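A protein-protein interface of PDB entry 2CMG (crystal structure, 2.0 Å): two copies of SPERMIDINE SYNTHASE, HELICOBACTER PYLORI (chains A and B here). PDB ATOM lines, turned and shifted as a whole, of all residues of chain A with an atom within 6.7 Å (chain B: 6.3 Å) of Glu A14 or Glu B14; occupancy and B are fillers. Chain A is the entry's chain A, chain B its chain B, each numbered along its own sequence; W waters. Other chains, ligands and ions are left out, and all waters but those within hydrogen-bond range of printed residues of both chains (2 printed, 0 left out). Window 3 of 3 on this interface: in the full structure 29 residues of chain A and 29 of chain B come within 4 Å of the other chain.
Tyr A10 touches Thr B16, and with the chains exchanged Thr A16 touches Tyr B10.
Leu A11 touches Glu B14, and with the chains exchanged Glu A14 touches Leu B11.
Leu A11 touches Tyr B15, and with the chains exchanged Tyr A15 touches Leu B11.
Lys A13 touches its own counterpart, Lys B13.
N of Tyr A15 sits at hydrogen-bond distance from O of Ile A3 (3.1 Å).
The side-chain amide oxygen (OE1) of Gln A5 sits at hydrogen-bond distance from the side-chain amino group (NZ) of Lys A13 (2.6 Å).
The side-chain hydroxyl of Tyr A15 sits at hydrogen-bond distance from the side-chain amide oxygen of Gln A5 (3.4 Å).
NZ of Lys A13 lies within hydrogen-bond range of OH of Tyr A15 (2.7 Å).
The backbone carbonyl oxygen (O) of Ile B3 sits at hydrogen-bond distance from the backbone NH (N) of Tyr B15, 3.0 Å away.
The side-chain amide nitrogen (NE2) of Gln B5 lies within hydrogen-bond range of the side-chain hydroxyl (OH) of Tyr B15 (2.6 Å).
Among the printed residues, merely in contact across the chains: Glu A14 with Leu B11 (3.1 Å), Arg A12 with Lys B13 (3.2 Å), Lys A13 with Arg B12 (3.4 Å), Leu A11 with Tyr B15 (3.4 Å), Tyr A15 with Leu B11 (3.4 Å), Tyr A10 with Tyr B15 (3.5 Å), Leu A11 with Glu B14 (3.5 Å), Tyr A15 with Tyr B10 (3.5 Å), Tyr A10 with Glu B14 (3.7 Å), Glu A14 with Tyr B10 (3.8 Å) and Lys A13 with Lys B13 (3.9 Å).
Of the 11 printed residues of chain B, 7 touch a printed residue of chain A.
Hydrophobic or aromatic side chains of chain B within 4 Å of the printed part of chain A: Tyr B10, Leu B11 and Tyr B15.
Printed residues of chain A that touch a printed residue of chain B: Tyr A10, Leu A11, Arg A12, Lys A13, Glu A14, Tyr A15 and Thr A16.
Among the printed residues, 16 pairs touch across the chains.
Water W2 bridges OE2 of Glu A14 and OE1 of Glu B14.
Water W1 lies within hydrogen-bond range of the side-chain carboxylate (OE2) of Glu A14 (3.0 Å) and the side-chain carboxylate (OE2) of Glu B14 (3.3 Å).
The backbone carbonyl oxygen of Tyr A10 sits at hydrogen-bond distance from the backbone NH of Thr B16 (3.0 Å).
The backbone carbonyl oxygen (O) of Arg A12 lies within hydrogen-bond range of the backbone NH (N) of Glu B14.
N of Glu A14 is in hydrogen-bond range of O of Arg B12 (2.6 Å).
The side-chain carboxylate of Glu A14 lies close to the side-chain carboxylate of Glu B14 (2.7 Å).
N of Thr A16 sits at hydrogen-bond distance from O of Tyr B10, at 3.1 Å.
Of the printed residues of chain B, Glu A14 touches Tyr B10, Leu B11, Arg B12 and Glu B14.
Glu B14 touches four residues of chain A.
Of the printed residues of chain B, Leu A11 touches Glu B14 and Tyr B15.
Of the printed residues of chain A, Leu B11 touches Glu A14 (3.1 Å) and Tyr A15 (3.4 Å).
Ile A3 touches none of the printed residues of chain B.
The nearest residue of chain B that does not touch Glu A14 is Lys B13 (4.8 Å).
The nearest residue of chain A that does not touch Glu B14 is Lys A13 (5.0 Å).
The nearest printed residue of chain A that does not touch Thr B16 is Arg A12 (4.4 Å).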
ATOM      1  N   TRP A   2      16.650  31.237  -1.506  1.00  0.00           N
ATOM      2  CA  TRP A   2      15.799  30.227  -0.893  1.00  0.00           C
ATOM      3  C   TRP A   2      14.455  30.092  -1.594  1.00  0.00           C
ATOM      4  O   TRP A   2      14.074  30.929  -2.412  1.00  0.00           O
ATOM      5  CB  TRP A   2      15.550  30.557   0.591  1.00  0.00           C
ATOM      6  CG  TRP A   2      15.146  31.994   0.868  1.00  0.00           C
ATOM      7  CD1 TRP A   2      15.985  33.047   1.081  1.00  0.00           C
ATOM      8  CD2 TRP A   2      13.812  32.527   0.916  1.00  0.00           C
ATOM      9  NE1 TRP A   2      15.261  34.206   1.261  1.00  0.00           N
ATOM     10  CE2 TRP A   2      13.927  33.918   1.165  1.00  0.00           C
ATOM     11  CE3 TRP A   2      12.533  31.973   0.775  1.00  0.00           C
ATOM     12  CZ2 TRP A   2      12.808  34.762   1.266  1.00  0.00           C
ATOM     13  CZ3 TRP A   2      11.418  32.811   0.875  1.00  0.00           C
ATOM     14  CH2 TRP A   2      11.565  34.191   1.122  1.00  0.00           C
ATOM     15  N   ILE A   3      13.755  29.011  -1.261  1.00  0.00           N
ATOM     16  CA  ILE A   3      12.431  28.729  -1.776  1.00  0.00           C
ATOM     17  C   ILE A   3      11.601  28.368  -0.550  1.00  0.00           C
ATOM     18  O   ILE A   3      12.053  27.615   0.316  1.00  0.00           O
ATOM     19  CB  ILE A   3      12.435  27.564  -2.807  1.00  0.00           C
ATOM     20  CG1 ILE A   3      12.927  26.262  -2.170  1.00  0.00           C
ATOM     21  CG2 ILE A   3      13.277  27.941  -3.998  1.00  0.00           C
ATOM     22  CD1 ILE A   3      12.633  24.998  -2.975  1.00  0.00           C
ATOM     23  N   THR A   4      10.401  28.940  -0.477  1.00  0.00           N
ATOM     24  CA  THR A   4       9.497  28.733   0.643  1.00  0.00           C
ATOM     25  C   THR A   4       8.397  27.706   0.380  1.00  0.00           C
ATOM     26  O   THR A   4       8.000  27.482  -0.763  1.00  0.00           O
ATOM     27  CB  THR A   4       8.830  30.073   1.057  1.00  0.00           C
ATOM     28  OG1 THR A   4       7.877  29.835   2.101  1.00  0.00           O
ATOM     29  CG2 THR A   4       8.116  30.715  -0.135  1.00  0.00           C
ATOM     30  N   GLN A   5       7.920  27.093   1.465  1.00  0.00           N
ATOM     31  CA  GLN A   5       6.856  26.094   1.424  1.00  0.00           C
ATOM     32  C   GLN A   5       5.922  26.355   2.603  1.00  0.00           C
ATOM     33  O   GLN A   5       6.355  26.382   3.753  1.00  0.00           O
ATOM     34  CB  GLN A   5       7.417  24.681   1.553  1.00  0.00           C
ATOM     35  CG  GLN A   5       6.541  23.651   0.857  1.00  0.00           C
ATOM     36  CD  GLN A   5       6.779  22.239   1.324  1.00  0.00           C
ATOM     37  OE1 GLN A   5       7.921  21.799   1.485  1.00  0.00           O
ATOM     38  NE2 GLN A   5       5.693  21.507   1.540  1.00  0.00           N
ATOM     39  N   TYR A  10       0.459  30.991   8.707  1.00  0.00           N
ATOM     40  CA  TYR A  10       1.335  31.621   9.686  1.00  0.00           C
ATOM     41  C   TYR A  10       2.525  30.717   9.983  1.00  0.00           C
ATOM     42  O   TYR A  10       3.242  30.909  10.968  1.00  0.00           O
ATOM     43  CB  TYR A  10       0.555  31.894  10.970  1.00  0.00           C
ATOM     44  CG  TYR A  10      -0.723  32.652  10.712  1.00  0.00           C
ATOM     45  CD1 TYR A  10      -0.688  33.952  10.219  1.00  0.00           C
ATOM     46  CD2 TYR A  10      -1.968  32.050  10.911  1.00  0.00           C
ATOM     47  CE1 TYR A  10      -1.861  34.638   9.925  1.00  0.00           C
ATOM     48  CE2 TYR A  10      -3.156  32.731  10.623  1.00  0.00           C
ATOM     49  CZ  TYR A  10      -3.088  34.025  10.129  1.00  0.00           C
ATOM     50  OH  TYR A  10      -4.241  34.714   9.834  1.00  0.00           O
ATOM     51  N   LEU A  11       2.727  29.720   9.133  1.00  0.00           N
ATOM     52  CA  LEU A  11       3.840  28.809   9.327  1.00  0.00           C
ATOM     53  C   LEU A  11       4.382  28.354   7.983  1.00  0.00           C
ATOM     54  O   LEU A  11       3.681  27.705   7.202  1.00  0.00           O
ATOM     55  CB  LEU A  11       3.397  27.614  10.157  1.00  0.00           C
ATOM     56  CG  LEU A  11       4.362  26.439  10.317  1.00  0.00           C
ATOM     57  CD1 LEU A  11       5.746  26.914  10.719  1.00  0.00           C
ATOM     58  CD2 LEU A  11       3.785  25.484  11.347  1.00  0.00           C
ATOM     59  N   ARG A  12       5.639  28.705   7.721  1.00  0.00           N
ATOM     60  CA  ARG A  12       6.311  28.354   6.468  1.00  0.00           C
ATOM     61  C   ARG A  12       7.638  27.644   6.723  1.00  0.00           C
ATOM     62  O   ARG A  12       8.180  27.699   7.817  1.00  0.00           O
ATOM     63  CB  ARG A  12       6.614  29.613   5.654  1.00  0.00           C
ATOM     64  CG  ARG A  12       5.422  30.445   5.218  1.00  0.00           C
ATOM     65  CD  ARG A  12       5.914  31.750   4.595  1.00  0.00           C
ATOM     66  NE  ARG A  12       4.841  32.597   4.073  1.00  0.00           N
ATOM     67  CZ  ARG A  12       3.825  33.055   4.798  1.00  0.00           C
ATOM     68  NH1 ARG A  12       3.722  32.743   6.089  1.00  0.00           N
ATOM     69  NH2 ARG A  12       2.926  33.853   4.239  1.00  0.00           N
ATOM     70  N   LYS A  13       8.152  26.987   5.689  1.00  0.00           N
ATOM     71  CA  LYS A  13       9.439  26.305   5.754  1.00  0.00           C
ATOM     72  C   LYS A  13      10.313  26.970   4.701  1.00  0.00           C
ATOM     73  O   LYS A  13       9.849  27.252   3.598  1.00  0.00           O
ATOM     74  CB  LYS A  13       9.324  24.809   5.434  1.00  0.00           C
ATOM     75  CG  LYS A  13       8.942  23.937   6.611  1.00  0.00           C
ATOM     76  CD  LYS A  13       9.081  22.450   6.308  1.00  0.00           C
ATOM     77  CE  LYS A  13       7.906  21.900   5.518  1.00  0.00           C
ATOM     78  NZ  LYS A  13       8.012  22.205   4.074  1.00  0.00           N
ATOM     79  N   GLU A  14      11.571  27.232   5.033  1.00  0.00           N
ATOM     80  CA  GLU A  14      12.469  27.879   4.082  1.00  0.00           C
ATOM     81  C   GLU A  14      13.675  26.966   3.824  1.00  0.00           C
ATOM     82  O   GLU A  14      14.392  26.586   4.767  1.00  0.00           O
ATOM     83  CB  GLU A  14      12.934  29.218   4.645  1.00  0.00           C
ATOM     84  CG  GLU A  14      11.835  30.048   5.310  1.00  0.00           C
ATOM     85  CD  GLU A  14      11.108  30.954   4.334  1.00  0.00           C
ATOM     86  OE1 GLU A  14      10.317  30.447   3.512  1.00  0.00           O
ATOM     87  OE2 GLU A  14      11.325  32.184   4.394  1.00  0.00           O
ATOM     88  N   TYR A  15      13.869  26.589   2.557  1.00  0.00           N
ATOM     89  CA  TYR A  15      14.968  25.698   2.154  1.00  0.00           C
ATOM     90  C   TYR A  15      16.066  26.383   1.344  1.00  0.00           C
ATOM     91  O   TYR A  15      15.912  26.540   0.125  1.00  0.00           O
ATOM     92  CB  TYR A  15      14.443  24.525   1.311  1.00  0.00           C
ATOM     93  CG  TYR A  15      13.411  23.650   1.978  1.00  0.00           C
ATOM     94  CD1 TYR A  15      12.095  24.069   2.089  1.00  0.00           C
ATOM     95  CD2 TYR A  15      13.736  22.370   2.438  1.00  0.00           C
ATOM     96  CE1 TYR A  15      11.116  23.231   2.629  1.00  0.00           C
ATOM     97  CE2 TYR A  15      12.761  21.529   2.983  1.00  0.00           C
ATOM     98  CZ  TYR A  15      11.458  21.967   3.069  1.00  0.00           C
ATOM     99  OH  TYR A  15      10.473  21.153   3.584  1.00  0.00           O
ATOM    100  N   THR A  16      17.178  26.752   1.987  1.00  0.00           N
ATOM    101  CA  THR A  16      18.272  27.406   1.267  1.00  0.00           C
ATOM    102  C   THR A  16      18.649  26.507   0.105  1.00  0.00           C
ATOM    103  O   THR A  16      18.672  25.286   0.245  1.00  0.00           O
ATOM    104  CB  THR A  16      19.525  27.609   2.165  1.00  0.00           C
ATOM    105  OG1 THR A  16      19.175  28.393   3.308  1.00  0.00           O
ATOM    106  CG2 THR A  16      20.629  28.348   1.396  1.00  0.00           C
ATOM    107  N   TRP B   2       7.728  38.084  13.162  1.00  0.00           N
ATOM    108  CA  TRP B   2       7.898  36.637  13.298  1.00  0.00           C
ATOM    109  C   TRP B   2       9.217  36.166  13.924  1.00  0.00           C
ATOM    110  O   TRP B   2      10.178  36.932  14.048  1.00  0.00           O
ATOM    111  CB  TRP B   2       7.723  35.961  11.933  1.00  0.00           C
ATOM    112  CG  TRP B   2       8.459  36.637  10.800  1.00  0.00           C
ATOM    113  CD1 TRP B   2       9.332  37.685  10.894  1.00  0.00           C
ATOM    114  CD2 TRP B   2       8.341  36.337   9.402  1.00  0.00           C
ATOM    115  NE1 TRP B   2       9.768  38.052   9.649  1.00  0.00           N
ATOM    116  CE2 TRP B   2       9.190  37.233   8.714  1.00  0.00           C
ATOM    117  CE3 TRP B   2       7.631  35.369   8.666  1.00  0.00           C
ATOM    118  CZ2 TRP B   2       9.312  37.230   7.317  1.00  0.00           C
ATOM    119  CZ3 TRP B   2       7.758  35.362   7.271  1.00  0.00           C
ATOM    120  CH2 TRP B   2       8.608  36.279   6.616  1.00  0.00           C
ATOM    121  N   ILE B   3       9.245  34.891  14.306  1.00  0.00           N
ATOM    122  CA  ILE B   3      10.418  34.278  14.921  1.00  0.00           C
ATOM    123  C   ILE B   3      10.753  33.038  14.082  1.00  0.00           C
ATOM    124  O   ILE B   3       9.922  32.590  13.289  1.00  0.00           O
ATOM    125  CB  ILE B   3      10.112  33.902  16.405  1.00  0.00           C
ATOM    126  CG1 ILE B   3      11.407  33.530  17.141  1.00  0.00           C
ATOM    127  CG2 ILE B   3       9.084  32.786  16.463  1.00  0.00           C
ATOM    128  CD1 ILE B   3      11.268  33.526  18.651  1.00  0.00           C
ATOM    129  N   THR B   4      11.952  32.481  14.229  1.00  0.00           N
ATOM    130  CA  THR B   4      12.304  31.307  13.428  1.00  0.00           C
ATOM    131  C   THR B   4      12.809  30.094  14.198  1.00  0.00           C
ATOM    132  O   THR B   4      13.550  30.229  15.175  1.00  0.00           O
ATOM    133  CB  THR B   4      13.362  31.655  12.330  1.00  0.00           C
ATOM    134  OG1 THR B   4      14.606  32.011  12.942  1.00  0.00           O
ATOM    135  CG2 THR B   4      12.880  32.814  11.476  1.00  0.00           C
ATOM    136  N   GLN B   5      12.398  28.911  13.745  1.00  0.00           N
ATOM    137  CA  GLN B   5      12.828  27.657  14.349  1.00  0.00           C
ATOM    138  C   GLN B   5      13.892  27.053  13.424  1.00  0.00           C
ATOM    139  O   GLN B   5      13.788  27.140  12.208  1.00  0.00           O
ATOM    140  CB  GLN B   5      11.650  26.684  14.497  1.00  0.00           C
ATOM    141  CG  GLN B   5      12.008  25.385  15.253  1.00  0.00           C
ATOM    142  CD  GLN B   5      10.835  24.413  15.409  1.00  0.00           C
ATOM    143  OE1 GLN B   5      10.792  23.617  16.355  1.00  0.00           O
ATOM    144  NE2 GLN B   5       9.891  24.466  14.476  1.00  0.00           N
ATOM    145  N   TYR B  10      20.204  24.598   6.745  1.00  0.00           N
ATOM    146  CA  TYR B  10      19.682  24.947   5.426  1.00  0.00           C
ATOM    147  C   TYR B  10      18.178  24.779   5.309  1.00  0.00           C
ATOM    148  O   TYR B  10      17.649  24.664   4.211  1.00  0.00           O
ATOM    149  CB  TYR B  10      20.354  24.118   4.334  1.00  0.00           C
ATOM    150  CG  TYR B  10      21.827  24.392   4.195  1.00  0.00           C
ATOM    151  CD1 TYR B  10      22.766  23.600   4.845  1.00  0.00           C
ATOM    152  CD2 TYR B  10      22.281  25.449   3.412  1.00  0.00           C
ATOM    153  CE1 TYR B  10      24.135  23.849   4.713  1.00  0.00           C
ATOM    154  CE2 TYR B  10      23.638  25.710   3.270  1.00  0.00           C
ATOM    155  CZ  TYR B  10      24.562  24.908   3.918  1.00  0.00           C
ATOM    156  OH  TYR B  10      25.905  25.144   3.738  1.00  0.00           O
ATOM    157  N   LEU B  11      17.501  24.763   6.452  1.00  0.00           N
ATOM    158  CA  LEU B  11      16.061  24.618   6.499  1.00  0.00           C
ATOM    159  C   LEU B  11      15.546  25.218   7.795  1.00  0.00           C
ATOM    160  O   LEU B  11      15.850  24.746   8.884  1.00  0.00           O
ATOM    161  CB  LEU B  11      15.674  23.147   6.413  1.00  0.00           C
ATOM    162  CG  LEU B  11      14.189  22.839   6.586  1.00  0.00           C
ATOM    163  CD1 LEU B  11      13.334  23.797   5.756  1.00  0.00           C
ATOM    164  CD2 LEU B  11      13.962  21.386   6.205  1.00  0.00           C
ATOM    165  N   ARG B  12      14.777  26.286   7.668  1.00  0.00           N
ATOM    166  CA  ARG B  12      14.229  26.954   8.831  1.00  0.00           C
ATOM    167  C   ARG B  12      12.731  27.098   8.701  1.00  0.00           C
ATOM    168  O   ARG B  12      12.187  27.134   7.594  1.00  0.00           O
ATOM    169  CB  ARG B  12      14.871  28.338   8.991  1.00  0.00           C
ATOM    170  CG  ARG B  12      16.338  28.293   9.369  1.00  0.00           C
ATOM    171  CD  ARG B  12      17.097  29.569   9.014  1.00  0.00           C
ATOM    172  NE  ARG B  12      18.436  29.559   9.600  1.00  0.00           N
ATOM    173  CZ  ARG B  12      19.224  28.486   9.635  1.00  0.00           C
ATOM    174  NH1 ARG B  12      18.806  27.336   9.119  1.00  0.00           N
ATOM    175  NH2 ARG B  12      20.433  28.552  10.187  1.00  0.00           N
ATOM    176  N   LYS B  13      12.072  27.162   9.849  1.00  0.00           N
ATOM    177  CA  LYS B  13      10.641  27.340   9.895  1.00  0.00           C
ATOM    178  C   LYS B  13      10.428  28.754  10.430  1.00  0.00           C
ATOM    179  O   LYS B  13      11.175  29.202  11.301  1.00  0.00           O
ATOM    180  CB  LYS B  13      10.033  26.299  10.825  1.00  0.00           C
ATOM    181  CG  LYS B  13      10.377  24.872  10.423  1.00  0.00           C
ATOM    182  CD  LYS B  13       9.866  23.884  11.446  1.00  0.00           C
ATOM    183  CE  LYS B  13       8.361  23.712  11.353  1.00  0.00           C
ATOM    184  NZ  LYS B  13       8.039  22.825  10.214  1.00  0.00           N
ATOM    185  N   GLU B  14       9.449  29.467   9.874  1.00  0.00           N
ATOM    186  CA  GLU B  14       9.140  30.829  10.303  1.00  0.00           C
ATOM    187  C   GLU B  14       7.685  30.899  10.770  1.00  0.00           C
ATOM    188  O   GLU B  14       6.767  30.616  10.005  1.00  0.00           O
ATOM    189  CB  GLU B  14       9.381  31.823   9.162  1.00  0.00           C
ATOM    190  CG  GLU B  14      10.742  31.649   8.507  1.00  0.00           C
ATOM    191  CD  GLU B  14      11.068  32.684   7.439  1.00  0.00           C
ATOM    192  OE1 GLU B  14      12.196  32.620   6.907  1.00  0.00           O
ATOM    193  OE2 GLU B  14      10.220  33.553   7.130  1.00  0.00           O
ATOM    194  N   TYR B  15       7.509  31.260  12.042  1.00  0.00           N
ATOM    195  CA  TYR B  15       6.207  31.379  12.696  1.00  0.00           C
ATOM    196  C   TYR B  15       5.816  32.838  12.829  1.00  0.00           C
ATOM    197  O   TYR B  15       6.592  33.632  13.348  1.00  0.00           O
ATOM    198  CB  TYR B  15       6.269  30.778  14.105  1.00  0.00           C
ATOM    199  CG  TYR B  15       6.569  29.300  14.139  1.00  0.00           C
ATOM    200  CD1 TYR B  15       5.540  28.358  14.143  1.00  0.00           C
ATOM    201  CD2 TYR B  15       7.886  28.838  14.145  1.00  0.00           C
ATOM    202  CE1 TYR B  15       5.813  26.991  14.152  1.00  0.00           C
ATOM    203  CE2 TYR B  15       8.172  27.474  14.149  1.00  0.00           C
ATOM    204  CZ  TYR B  15       7.131  26.559  14.152  1.00  0.00           C
ATOM    205  OH  TYR B  15       7.408  25.213  14.144  1.00  0.00           O
ATOM    206  N   THR B  16       4.616  33.185  12.357  1.00  0.00           N
ATOM    207  CA  THR B  16       4.116  34.557  12.458  1.00  0.00           C
ATOM    208  C   THR B  16       3.489  34.689  13.838  1.00  0.00           C
ATOM    209  O   THR B  16       2.709  33.836  14.251  1.00  0.00           O
ATOM    210  CB  THR B  16       3.024  34.854  11.429  1.00  0.00           C
ATOM    211  OG1 THR B  16       3.476  34.463  10.131  1.00  0.00           O
ATOM    212  CG2 THR B  16       2.677  36.347  11.428  1.00  0.00           C
HETATM  213  O   HOH W   1       8.749  33.803   4.181  1.00  0.00           O
HETATM  214  O   HOH W   2      13.988  33.168   4.461  1.00  0.00           O
